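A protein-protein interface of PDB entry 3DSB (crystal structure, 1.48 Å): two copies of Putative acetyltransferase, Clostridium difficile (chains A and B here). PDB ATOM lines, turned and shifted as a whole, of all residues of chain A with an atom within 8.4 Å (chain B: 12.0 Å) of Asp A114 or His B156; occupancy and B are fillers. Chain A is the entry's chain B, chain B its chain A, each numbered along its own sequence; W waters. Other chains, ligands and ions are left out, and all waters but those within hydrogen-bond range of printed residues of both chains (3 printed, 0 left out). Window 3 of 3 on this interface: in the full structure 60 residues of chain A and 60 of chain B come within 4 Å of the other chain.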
ATOM      1  N   GLY A  82      -3.956  16.952   1.922  1.00  0.00           N
ATOM      2  CA  GLY A  82      -3.327  17.049   3.236  1.00  0.00           C
ATOM      3  C   GLY A  82      -4.291  17.624   4.241  1.00  0.00           C
ATOM      4  O   GLY A  82      -5.405  17.967   3.896  1.00  0.00           O
ATOM      5  N   ASN A  83      -3.850  17.734   5.493  1.00  0.00           N
ATOM      6  CA  ASN A  83      -4.689  18.231   6.573  1.00  0.00           C
ATOM      7  C   ASN A  83      -4.424  19.694   6.837  1.00  0.00           C
ATOM      8  O   ASN A  83      -3.247  20.135   6.855  1.00  0.00           O
ATOM      9  CB  ASN A  83      -4.368  17.496   7.867  1.00  0.00           C
ATOM     10  CG  ASN A  83      -5.047  16.152   7.960  1.00  0.00           C
ATOM     11  OD1 ASN A  83      -6.272  16.043   7.877  1.00  0.00           O
ATOM     12  ND2 ASN A  83      -4.250  15.099   8.177  1.00  0.00           N
ATOM     13  N   LEU A  85      -4.501  21.865  10.156  1.00  0.00           N
ATOM     14  CA  LEU A  85      -4.663  21.773  11.612  1.00  0.00           C
ATOM     15  C   LEU A  85      -5.470  22.973  12.088  1.00  0.00           C
ATOM     16  O   LEU A  85      -5.172  24.110  11.696  1.00  0.00           O
ATOM     17  CB  LEU A  85      -3.305  21.810  12.328  1.00  0.00           C
ATOM     18  CG  LEU A  85      -2.593  20.486  12.572  1.00  0.00           C
ATOM     19  CD1 LEU A  85      -2.611  19.528  11.422  1.00  0.00           C
ATOM     20  CD2 LEU A  85      -1.203  20.692  13.222  1.00  0.00           C
ATOM     21  N   ASN A 107       4.183  28.401  18.506  1.00  0.00           N
ATOM     22  CA  ASN A 107       5.301  28.271  17.607  1.00  0.00           C
ATOM     23  C   ASN A 107       5.685  26.800  17.440  1.00  0.00           C
ATOM     24  O   ASN A 107       6.160  26.395  16.375  1.00  0.00           O
ATOM     25  CB  ASN A 107       6.449  29.173  18.044  1.00  0.00           C
ATOM     26  CG  ASN A 107       6.213  30.622  17.650  1.00  0.00           C
ATOM     27  OD1 ASN A 107       5.691  30.906  16.546  1.00  0.00           O
ATOM     28  ND2 ASN A 107       6.559  31.540  18.520  1.00  0.00           N
ATOM     29  N   TYR A 108       5.470  26.005  18.492  1.00  0.00           N
ATOM     30  CA  TYR A 108       5.723  24.568  18.399  1.00  0.00           C
ATOM     31  C   TYR A 108       4.795  23.941  17.354  1.00  0.00           C
ATOM     32  O   TYR A 108       5.200  23.092  16.568  1.00  0.00           O
ATOM     33  CB  TYR A 108       5.477  23.909  19.756  1.00  0.00           C
ATOM     34  CG  TYR A 108       5.981  22.489  19.868  1.00  0.00           C
ATOM     35  CD1 TYR A 108       7.297  22.258  20.256  1.00  0.00           C
ATOM     36  CD2 TYR A 108       5.157  21.401  19.627  1.00  0.00           C
ATOM     37  CE1 TYR A 108       7.794  20.960  20.391  1.00  0.00           C
ATOM     38  CE2 TYR A 108       5.647  20.070  19.740  1.00  0.00           C
ATOM     39  CZ  TYR A 108       6.965  19.882  20.139  1.00  0.00           C
ATOM     40  OH  TYR A 108       7.466  18.608  20.275  1.00  0.00           O
ATOM     41  N   ILE A 109       3.521  24.344  17.357  1.00  0.00           N
ATOM     42  CA  ILE A 109       2.574  23.837  16.354  1.00  0.00           C
ATOM     43  C   ILE A 109       2.917  24.362  14.952  1.00  0.00           C
ATOM     44  O   ILE A 109       2.823  23.599  13.985  1.00  0.00           O
ATOM     45  CB  ILE A 109       1.107  24.167  16.740  1.00  0.00           C
ATOM     46  CG1 ILE A 109       0.795  23.681  18.169  1.00  0.00           C
ATOM     47  CG2 ILE A 109       0.137  23.543  15.758  1.00  0.00           C
ATOM     48  CD1 ILE A 109       1.056  22.233  18.427  1.00  0.00           C
ATOM     49  N   LYS A 110       3.305  25.631  14.837  1.00  0.00           N
ATOM     50  CA  LYS A 110       3.716  26.172  13.538  1.00  0.00           C
ATOM     51  C   LYS A 110       4.855  25.319  12.947  1.00  0.00           C
ATOM     52  O   LYS A 110       4.867  25.011  11.747  1.00  0.00           O
ATOM     53  CB  LYS A 110       4.151  27.647  13.635  1.00  0.00           C
ATOM     54  CG  LYS A 110       2.975  28.614  13.842  1.00  0.00           C
ATOM     55  CD  LYS A 110       3.362  29.993  14.421  1.00  0.00           C
ATOM     56  CE  LYS A 110       4.265  30.813  13.525  1.00  0.00           C
ATOM     57  NZ  LYS A 110       4.561  32.155  14.175  1.00  0.00           N
ATOM     58  N   ASN A 111       5.822  24.959  13.796  1.00  0.00           N
ATOM     59  CA  ASN A 111       6.920  24.105  13.352  1.00  0.00           C
ATOM     60  C   ASN A 111       6.435  22.742  12.927  1.00  0.00           C
ATOM     61  O   ASN A 111       6.881  22.252  11.888  1.00  0.00           O
ATOM     62  CB  ASN A 111       7.952  23.968  14.476  1.00  0.00           C
ATOM     63  CG  ASN A 111       9.118  23.089  14.070  1.00  0.00           C
ATOM     64  OD1 ASN A 111       9.268  21.978  14.573  1.00  0.00           O
ATOM     65  ND2 ASN A 111       9.904  23.559  13.127  1.00  0.00           N
ATOM     66  N   ILE A 112       5.549  22.108  13.706  1.00  0.00           N
ATOM     67  CA  ILE A 112       4.946  20.828  13.270  1.00  0.00           C
ATOM     68  C   ILE A 112       4.373  20.959  11.863  1.00  0.00           C
ATOM     69  O   ILE A 112       4.633  20.125  11.000  1.00  0.00           O
ATOM     70  CB  ILE A 112       3.860  20.293  14.239  1.00  0.00           C
ATOM     71  CG1 ILE A 112       4.504  19.707  15.505  1.00  0.00           C
ATOM     72  CG2 ILE A 112       2.859  19.289  13.546  1.00  0.00           C
ATOM     73  CD1 ILE A 112       3.556  19.458  16.643  1.00  0.00           C
ATOM     74  N   CYS A 113       3.628  22.029  11.616  1.00  0.00           N
ATOM     75  CA  CYS A 113       3.037  22.253  10.267  1.00  0.00           C
ATOM     76  C   CYS A 113       4.110  22.431   9.178  1.00  0.00           C
ATOM     77  O   CYS A 113       4.009  21.834   8.087  1.00  0.00           O
ATOM     78  CB  CYS A 113       2.133  23.477  10.295  1.00  0.00           C
ATOM     79  SG  CYS A 113       0.684  23.252  11.364  1.00  0.00           S
ATOM     80  N   ASP A 114       5.138  23.236   9.465  1.00  0.00           N
ATOM     81  CA  ASP A 114       6.170  23.562   8.467  1.00  0.00           C
ATOM     82  C   ASP A 114       6.984  22.324   8.075  1.00  0.00           C
ATOM     83  O   ASP A 114       7.402  22.206   6.912  1.00  0.00           O
ATOM     84  CB  ASP A 114       7.111  24.647   8.999  1.00  0.00           C
ATOM     85  CG  ASP A 114       6.470  26.008   9.063  1.00  0.00           C
ATOM     86  OD1 ASP A 114       5.431  26.222   8.400  1.00  0.00           O
ATOM     87  OD2 ASP A 114       7.034  26.871   9.745  1.00  0.00           O
ATOM     88  N   LYS A 115       7.187  21.425   9.040  1.00  0.00           N
ATOM     89  CA  LYS A 115       8.031  20.207   8.918  1.00  0.00           C
ATOM     90  C   LYS A 115       7.246  18.961   8.496  1.00  0.00           C
ATOM     91  O   LYS A 115       7.740  17.798   8.560  1.00  0.00           O
ATOM     92  CB  LYS A 115       8.694  19.881  10.270  1.00  0.00           C
ATOM     93  CG  LYS A 115       9.691  20.886  10.772  1.00  0.00           C
ATOM     94  CD  LYS A 115      10.712  21.251   9.722  1.00  0.00           C
ATOM     95  CE  LYS A 115      11.707  22.240  10.298  1.00  0.00           C
ATOM     96  NZ  LYS A 115      12.309  21.686  11.525  1.00  0.00           N
ATOM     97  N   ASP A 116       5.994  19.150   8.100  1.00  0.00           N
ATOM     98  CA  ASP A 116       5.243  18.004   7.659  1.00  0.00           C
ATOM     99  C   ASP A 116       4.549  18.364   6.354  1.00  0.00           C
ATOM    100  O   ASP A 116       3.576  19.088   6.357  1.00  0.00           O
ATOM    101  CB  ASP A 116       4.261  17.574   8.755  1.00  0.00           C
ATOM    102  CG  ASP A 116       3.448  16.365   8.379  1.00  0.00           C
ATOM    103  OD1 ASP A 116       3.422  16.013   7.182  1.00  0.00           O
ATOM    104  OD2 ASP A 116       2.836  15.747   9.277  1.00  0.00           O
ATOM    105  N   GLU A 117       5.068  17.909   5.222  1.00  0.00           N
ATOM    106  CA  GLU A 117       4.431  18.203   3.939  1.00  0.00           C
ATOM    107  C   GLU A 117       3.002  17.621   3.820  1.00  0.00           C
ATOM    108  O   GLU A 117       2.274  17.940   2.885  1.00  0.00           O
ATOM    109  CB  GLU A 117       5.346  17.793   2.765  1.00  0.00           C
ATOM    110  CG  GLU A 117       6.639  18.625   2.678  1.00  0.00           C
ATOM    111  CD  GLU A 117       7.602  18.163   1.585  1.00  0.00           C
ATOM    112  OE1 GLU A 117       7.331  17.146   0.909  1.00  0.00           O
ATOM    113  OE2 GLU A 117       8.644  18.825   1.409  1.00  0.00           O
ATOM    114  N   ASN A 118       2.591  16.770   4.773  1.00  0.00           N
ATOM    115  CA  ASN A 118       1.199  16.233   4.830  1.00  0.00           C
ATOM    116  C   ASN A 118       0.221  17.189   5.597  1.00  0.00           C
ATOM    117  O   ASN A 118      -0.996  16.930   5.749  1.00  0.00           O
ATOM    118  CB  ASN A 118       1.207  14.828   5.444  1.00  0.00           C
ATOM    119  CG  ASN A 118      -0.199  14.261   5.718  1.00  0.00           C
ATOM    120  OD1 ASN A 118      -0.976  13.908   4.790  1.00  0.00           O
ATOM    121  ND2 ASN A 118      -0.516  14.124   7.000  1.00  0.00           N
ATOM    122  N   ILE A 119       0.773  18.290   6.084  1.00  0.00           N
ATOM    123  CA  ILE A 119      -0.040  19.378   6.666  1.00  0.00           C
ATOM    124  C   ILE A 119       0.016  20.543   5.713  1.00  0.00           C
ATOM    125  O   ILE A 119       1.090  20.983   5.292  1.00  0.00           O
ATOM    126  CB  ILE A 119       0.497  19.815   8.061  1.00  0.00           C
ATOM    127  CG1 ILE A 119       0.213  18.695   9.043  1.00  0.00           C
ATOM    128  CG2 ILE A 119      -0.177  21.161   8.504  1.00  0.00           C
ATOM    129  CD1 ILE A 119       0.823  18.890  10.451  1.00  0.00           C
ATOM    130  N   VAL A 120      -1.158  21.011   5.298  1.00  0.00           N
ATOM    131  CA  VAL A 120      -1.207  22.045   4.268  1.00  0.00           C
ATOM    132  C   VAL A 120      -1.644  23.432   4.762  1.00  0.00           C
ATOM    133  O   VAL A 120      -1.692  24.393   3.999  1.00  0.00           O
ATOM    134  CB  VAL A 120      -2.095  21.607   3.088  1.00  0.00           C
ATOM    135  CG1 VAL A 120      -1.496  20.334   2.404  1.00  0.00           C
ATOM    136  CG2 VAL A 120      -3.520  21.400   3.554  1.00  0.00           C
ATOM    137  N   GLY A 121      -1.957  23.541   6.038  1.00  0.00           N
ATOM    138  CA  GLY A 121      -2.329  24.856   6.570  1.00  0.00           C
ATOM    139  C   GLY A 121      -2.631  24.753   8.041  1.00  0.00           C
ATOM    140  O   GLY A 121      -2.695  23.637   8.603  1.00  0.00           O
ATOM    141  N   MET A 122      -2.844  25.912   8.673  1.00  0.00           N
ATOM    142  CA  MET A 122      -3.021  25.973  10.124  1.00  0.00           C
ATOM    143  C   MET A 122      -3.994  27.108  10.355  1.00  0.00           C
ATOM    144  O   MET A 122      -3.724  28.254   9.968  1.00  0.00           O
ATOM    145  CB  MET A 122      -1.679  26.283  10.813  1.00  0.00           C
ATOM    146  CG  MET A 122      -1.802  26.267  12.291  1.00  0.00           C
ATOM    147  SD  MET A 122      -0.114  26.601  13.171  1.00  0.00           S
ATOM    148  CE  MET A 122      -0.611  28.342  13.862  1.00  0.00           C
ATOM    149  N   VAL B  40      -2.676  15.979  -7.496  1.00  0.00           N
ATOM    150  CA  VAL B  40      -2.894  16.217  -6.074  1.00  0.00           C
ATOM    151  C   VAL B  40      -4.330  15.900  -5.653  1.00  0.00           C
ATOM    152  O   VAL B  40      -4.560  15.217  -4.637  1.00  0.00           O
ATOM    153  CB  VAL B  40      -2.553  17.687  -5.722  1.00  0.00           C
ATOM    154  CG1 VAL B  40      -2.908  18.011  -4.293  1.00  0.00           C
ATOM    155  CG2 VAL B  40      -1.073  17.970  -6.017  1.00  0.00           C
ATOM    156  N   GLU B 151      -5.311  32.409   9.911  1.00  0.00           N
ATOM    157  CA  GLU B 151      -4.458  31.320   9.448  1.00  0.00           C
ATOM    158  C   GLU B 151      -3.000  31.719   9.424  1.00  0.00           C
ATOM    159  O   GLU B 151      -2.652  32.920   9.289  1.00  0.00           O
ATOM    160  CB  GLU B 151      -4.900  30.832   8.079  1.00  0.00           C
ATOM    161  CG  GLU B 151      -4.524  31.741   6.946  1.00  0.00           C
ATOM    162  CD  GLU B 151      -5.027  31.241   5.602  1.00  0.00           C
ATOM    163  OE1 GLU B 151      -5.291  30.010   5.458  1.00  0.00           O
ATOM    164  OE2 GLU B 151      -5.079  32.060   4.650  1.00  0.00           O
ATOM    165  N   TYR B 152      -2.166  30.700   9.544  1.00  0.00           N
ATOM    166  CA  TYR B 152      -0.737  30.871   9.414  1.00  0.00           C
ATOM    167  C   TYR B 152      -0.351  30.286   8.067  1.00  0.00           C
ATOM    168  O   TYR B 152      -0.783  29.170   7.728  1.00  0.00           O
ATOM    169  CB  TYR B 152      -0.007  30.146  10.560  1.00  0.00           C
ATOM    170  CG  TYR B 152       1.475  29.869  10.296  1.00  0.00           C
ATOM    171  CD1 TYR B 152       2.393  30.917  10.186  1.00  0.00           C
ATOM    172  CD2 TYR B 152       1.944  28.549  10.183  1.00  0.00           C
ATOM    173  CE1 TYR B 152       3.753  30.659   9.935  1.00  0.00           C
ATOM    174  CE2 TYR B 152       3.306  28.274   9.940  1.00  0.00           C
ATOM    175  CZ  TYR B 152       4.189  29.331   9.810  1.00  0.00           C
ATOM    176  OH  TYR B 152       5.519  29.065   9.564  1.00  0.00           O
ATOM    177  N   GLU B 153       0.478  31.021   7.325  1.00  0.00           N
ATOM    178  CA  GLU B 153       0.904  30.575   6.004  1.00  0.00           C
ATOM    179  C   GLU B 153       2.023  29.551   6.180  1.00  0.00           C
ATOM    180  O   GLU B 153       3.166  29.921   6.456  1.00  0.00           O
ATOM    181  CB  GLU B 153       1.385  31.781   5.198  1.00  0.00           C
ATOM    182  CG  GLU B 153       1.884  31.491   3.787  1.00  0.00           C
ATOM    183  CD  GLU B 153       0.760  31.109   2.822  1.00  0.00           C
ATOM    184  OE1 GLU B 153      -0.437  31.383   3.130  1.00  0.00           O
ATOM    185  OE2 GLU B 153       1.092  30.535   1.751  1.00  0.00           O
ATOM    186  N   VAL B 154       1.675  28.281   6.071  1.00  0.00           N
ATOM    187  CA  VAL B 154       2.660  27.217   6.292  1.00  0.00           C
ATOM    188  C   VAL B 154       3.734  27.326   5.193  1.00  0.00           C
ATOM    189  O   VAL B 154       3.402  27.326   4.004  1.00  0.00           O
ATOM    190  CB  VAL B 154       1.942  25.850   6.388  1.00  0.00           C
ATOM    191  CG1 VAL B 154       2.919  24.718   6.415  1.00  0.00           C
ATOM    192  CG2 VAL B 154       1.049  25.820   7.638  1.00  0.00           C
ATOM    193  N   ILE B 155       4.993  27.524   5.607  1.00  0.00           N
ATOM    194  CA  ILE B 155       6.100  27.689   4.653  1.00  0.00           C
ATOM    195  C   ILE B 155       6.660  26.316   4.423  1.00  0.00           C
ATOM    196  O   ILE B 155       7.354  25.754   5.276  1.00  0.00           O
ATOM    197  CB  ILE B 155       7.195  28.706   5.104  1.00  0.00           C
ATOM    198  CG1 ILE B 155       6.601  30.125   5.218  1.00  0.00           C
ATOM    199  CG2 ILE B 155       8.410  28.691   4.110  1.00  0.00           C
ATOM    200  CD1 ILE B 155       5.778  30.556   3.998  1.00  0.00           C
ATOM    201  N   HIS B 156       6.334  25.784   3.253  1.00  0.00           N
ATOM    202  CA  HIS B 156       6.433  24.377   3.117  1.00  0.00           C
ATOM    203  C   HIS B 156       7.744  23.670   2.943  1.00  0.00           C
ATOM    204  O   HIS B 156       8.274  23.215   3.959  1.00  0.00           O
ATOM    205  CB  HIS B 156       5.222  23.670   2.544  1.00  0.00           C
ATOM    206  CG  HIS B 156       4.644  22.755   3.557  1.00  0.00           C
ATOM    207  ND1 HIS B 156       5.407  22.311   4.614  1.00  0.00           N
ATOM    208  CD2 HIS B 156       3.411  22.230   3.733  1.00  0.00           C
ATOM    209  CE1 HIS B 156       4.676  21.534   5.388  1.00  0.00           C
ATOM    210  NE2 HIS B 156       3.463  21.470   4.880  1.00  0.00           N
HETATM  211  O   HOH W   1       2.710  20.201   1.993  1.00  0.00           O
HETATM  212  O   HOH W   2      -0.832  27.299   4.568  1.00  0.00           O
HETATM  213  O   HOH W   3      -2.987  27.944   6.585  1.00  0.00           O
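A ring nitrogen (NE2) of His B156 sits close to the backbone carbonyl oxygen (O) of Cys A113. The backbone NH (N) of Tyr B152 sits at hydrogen-bond distance from the backbone carbonyl oxygen (O) of Met A122, at 2.9 Å. The backbone NH of Ile B155 lies within hydrogen-bond range of the side-chain carboxylate of Asp A114 (3.1 Å). OH of Tyr B152 sits at hydrogen-bond distance from OD2 of Asp A114 (2.7 Å). O of Asp A116 sits at hydrogen-bond distance from NE2 of His B156 (2.8 Å). A ring nitrogen (ND1) of His B156 is in hydrogen-bond range of the backbone carbonyl oxygen (O) of Asp A114, 3.0 Å away. O of Ile A119 is in hydrogen-bond range of NE2 of His B156.
The backbone NH of Leu A85 is in hydrogen-bond range of the backbone carbonyl oxygen of Gly A121, 3.0 Å away. The side-chain carboxylate (OD1) of Asp A116 lies within hydrogen-bond range of the backbone NH (N) of Asn A118, 2.7 Å away. The side-chain amino group (NZ) of Lys A110 is in hydrogen-bond range of the side-chain amide oxygen (OD1) of Asn A107 (2.9 Å). The side-chain sulfur (SG) of Cys A113 lies within hydrogen-bond range of the backbone carbonyl oxygen (O) of Ile A109 (3.4 Å).
Tyr B152 touches Lys A110. Cys A113 touches Val B154. OD1 of Asp A114 touches CG1 of Val B154 (3.5 Å). His B156 touches Glu A117 (NE2 to CA, 3.5 Å). CG2 of Val B154 touches CA of Gly A121, 3.7 Å away. Met A122 touches Glu B151.
Of the printed residues of chain B, Lys A110 touches Tyr B152. No residue of chain B comes within 4 Å of Asn A111. Cys A113 touches just these residues of chain B: Val B154 (3.5 Å) and His B156 (2.8 Å). No residue of chain B comes within 4 Å of Lys A115. Asp A116 touches one residue of chain B. Of the printed residues of chain B, Glu A117 touches His B156. Asn A118 touches none of the printed residues of chain B. No residue of chain B comes within 4 Å of Val A120. Gly A121 touches just one residue of chain B: Val B154 (3.7 Å). Of the printed residues of chain A, Tyr B152 touches Lys A110 (3.6 Å), Asp A114 (2.7 Å) and Met A122 (2.9 Å). Of the printed residues of chain A, His B156 touches Cys A113, Asp A114, Asp A116, Glu A117 and Ile A119. The nearest residue of chain B that does not touch Asp A114 is Glu B153 (4.8 Å). The nearest printed residue of chain B that does not touch Met A122 is Val B154 (4.03 Å).
Printed residues of chain B that touch a printed residue of chain A: Glu B151, Tyr B152, Val B154, Ile B155 and His B156. Hydrophobic or aromatic side chains of chain B that line the printed part of chain A: Tyr B152, Val B154 and His B156. Hydrophobic or aromatic side chains of chain A within 4 Å of the printed part of chain B: Met A122. Among the printed residues, 13 pairs touch across the chains. Among the printed residues, no Asp or Glu carboxylate lies within 4 Å of a Lys or Arg side-chain nitrogen of the other chain.
No position is printed for both chains.
Water W1 bridges O of Glu A117 (2.5 Å) and NE2 of His B156 (3.2 Å). Water W3 lies within hydrogen-bond range of O of Tyr B152, N of Met A122 and OE1 of Glu B151. Water W2 lies within hydrogen-bond range of the backbone NH (N) of Val B154 (3.1 Å) and the backbone carbonyl oxygen (O) of Val A120 (3.1 Å).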
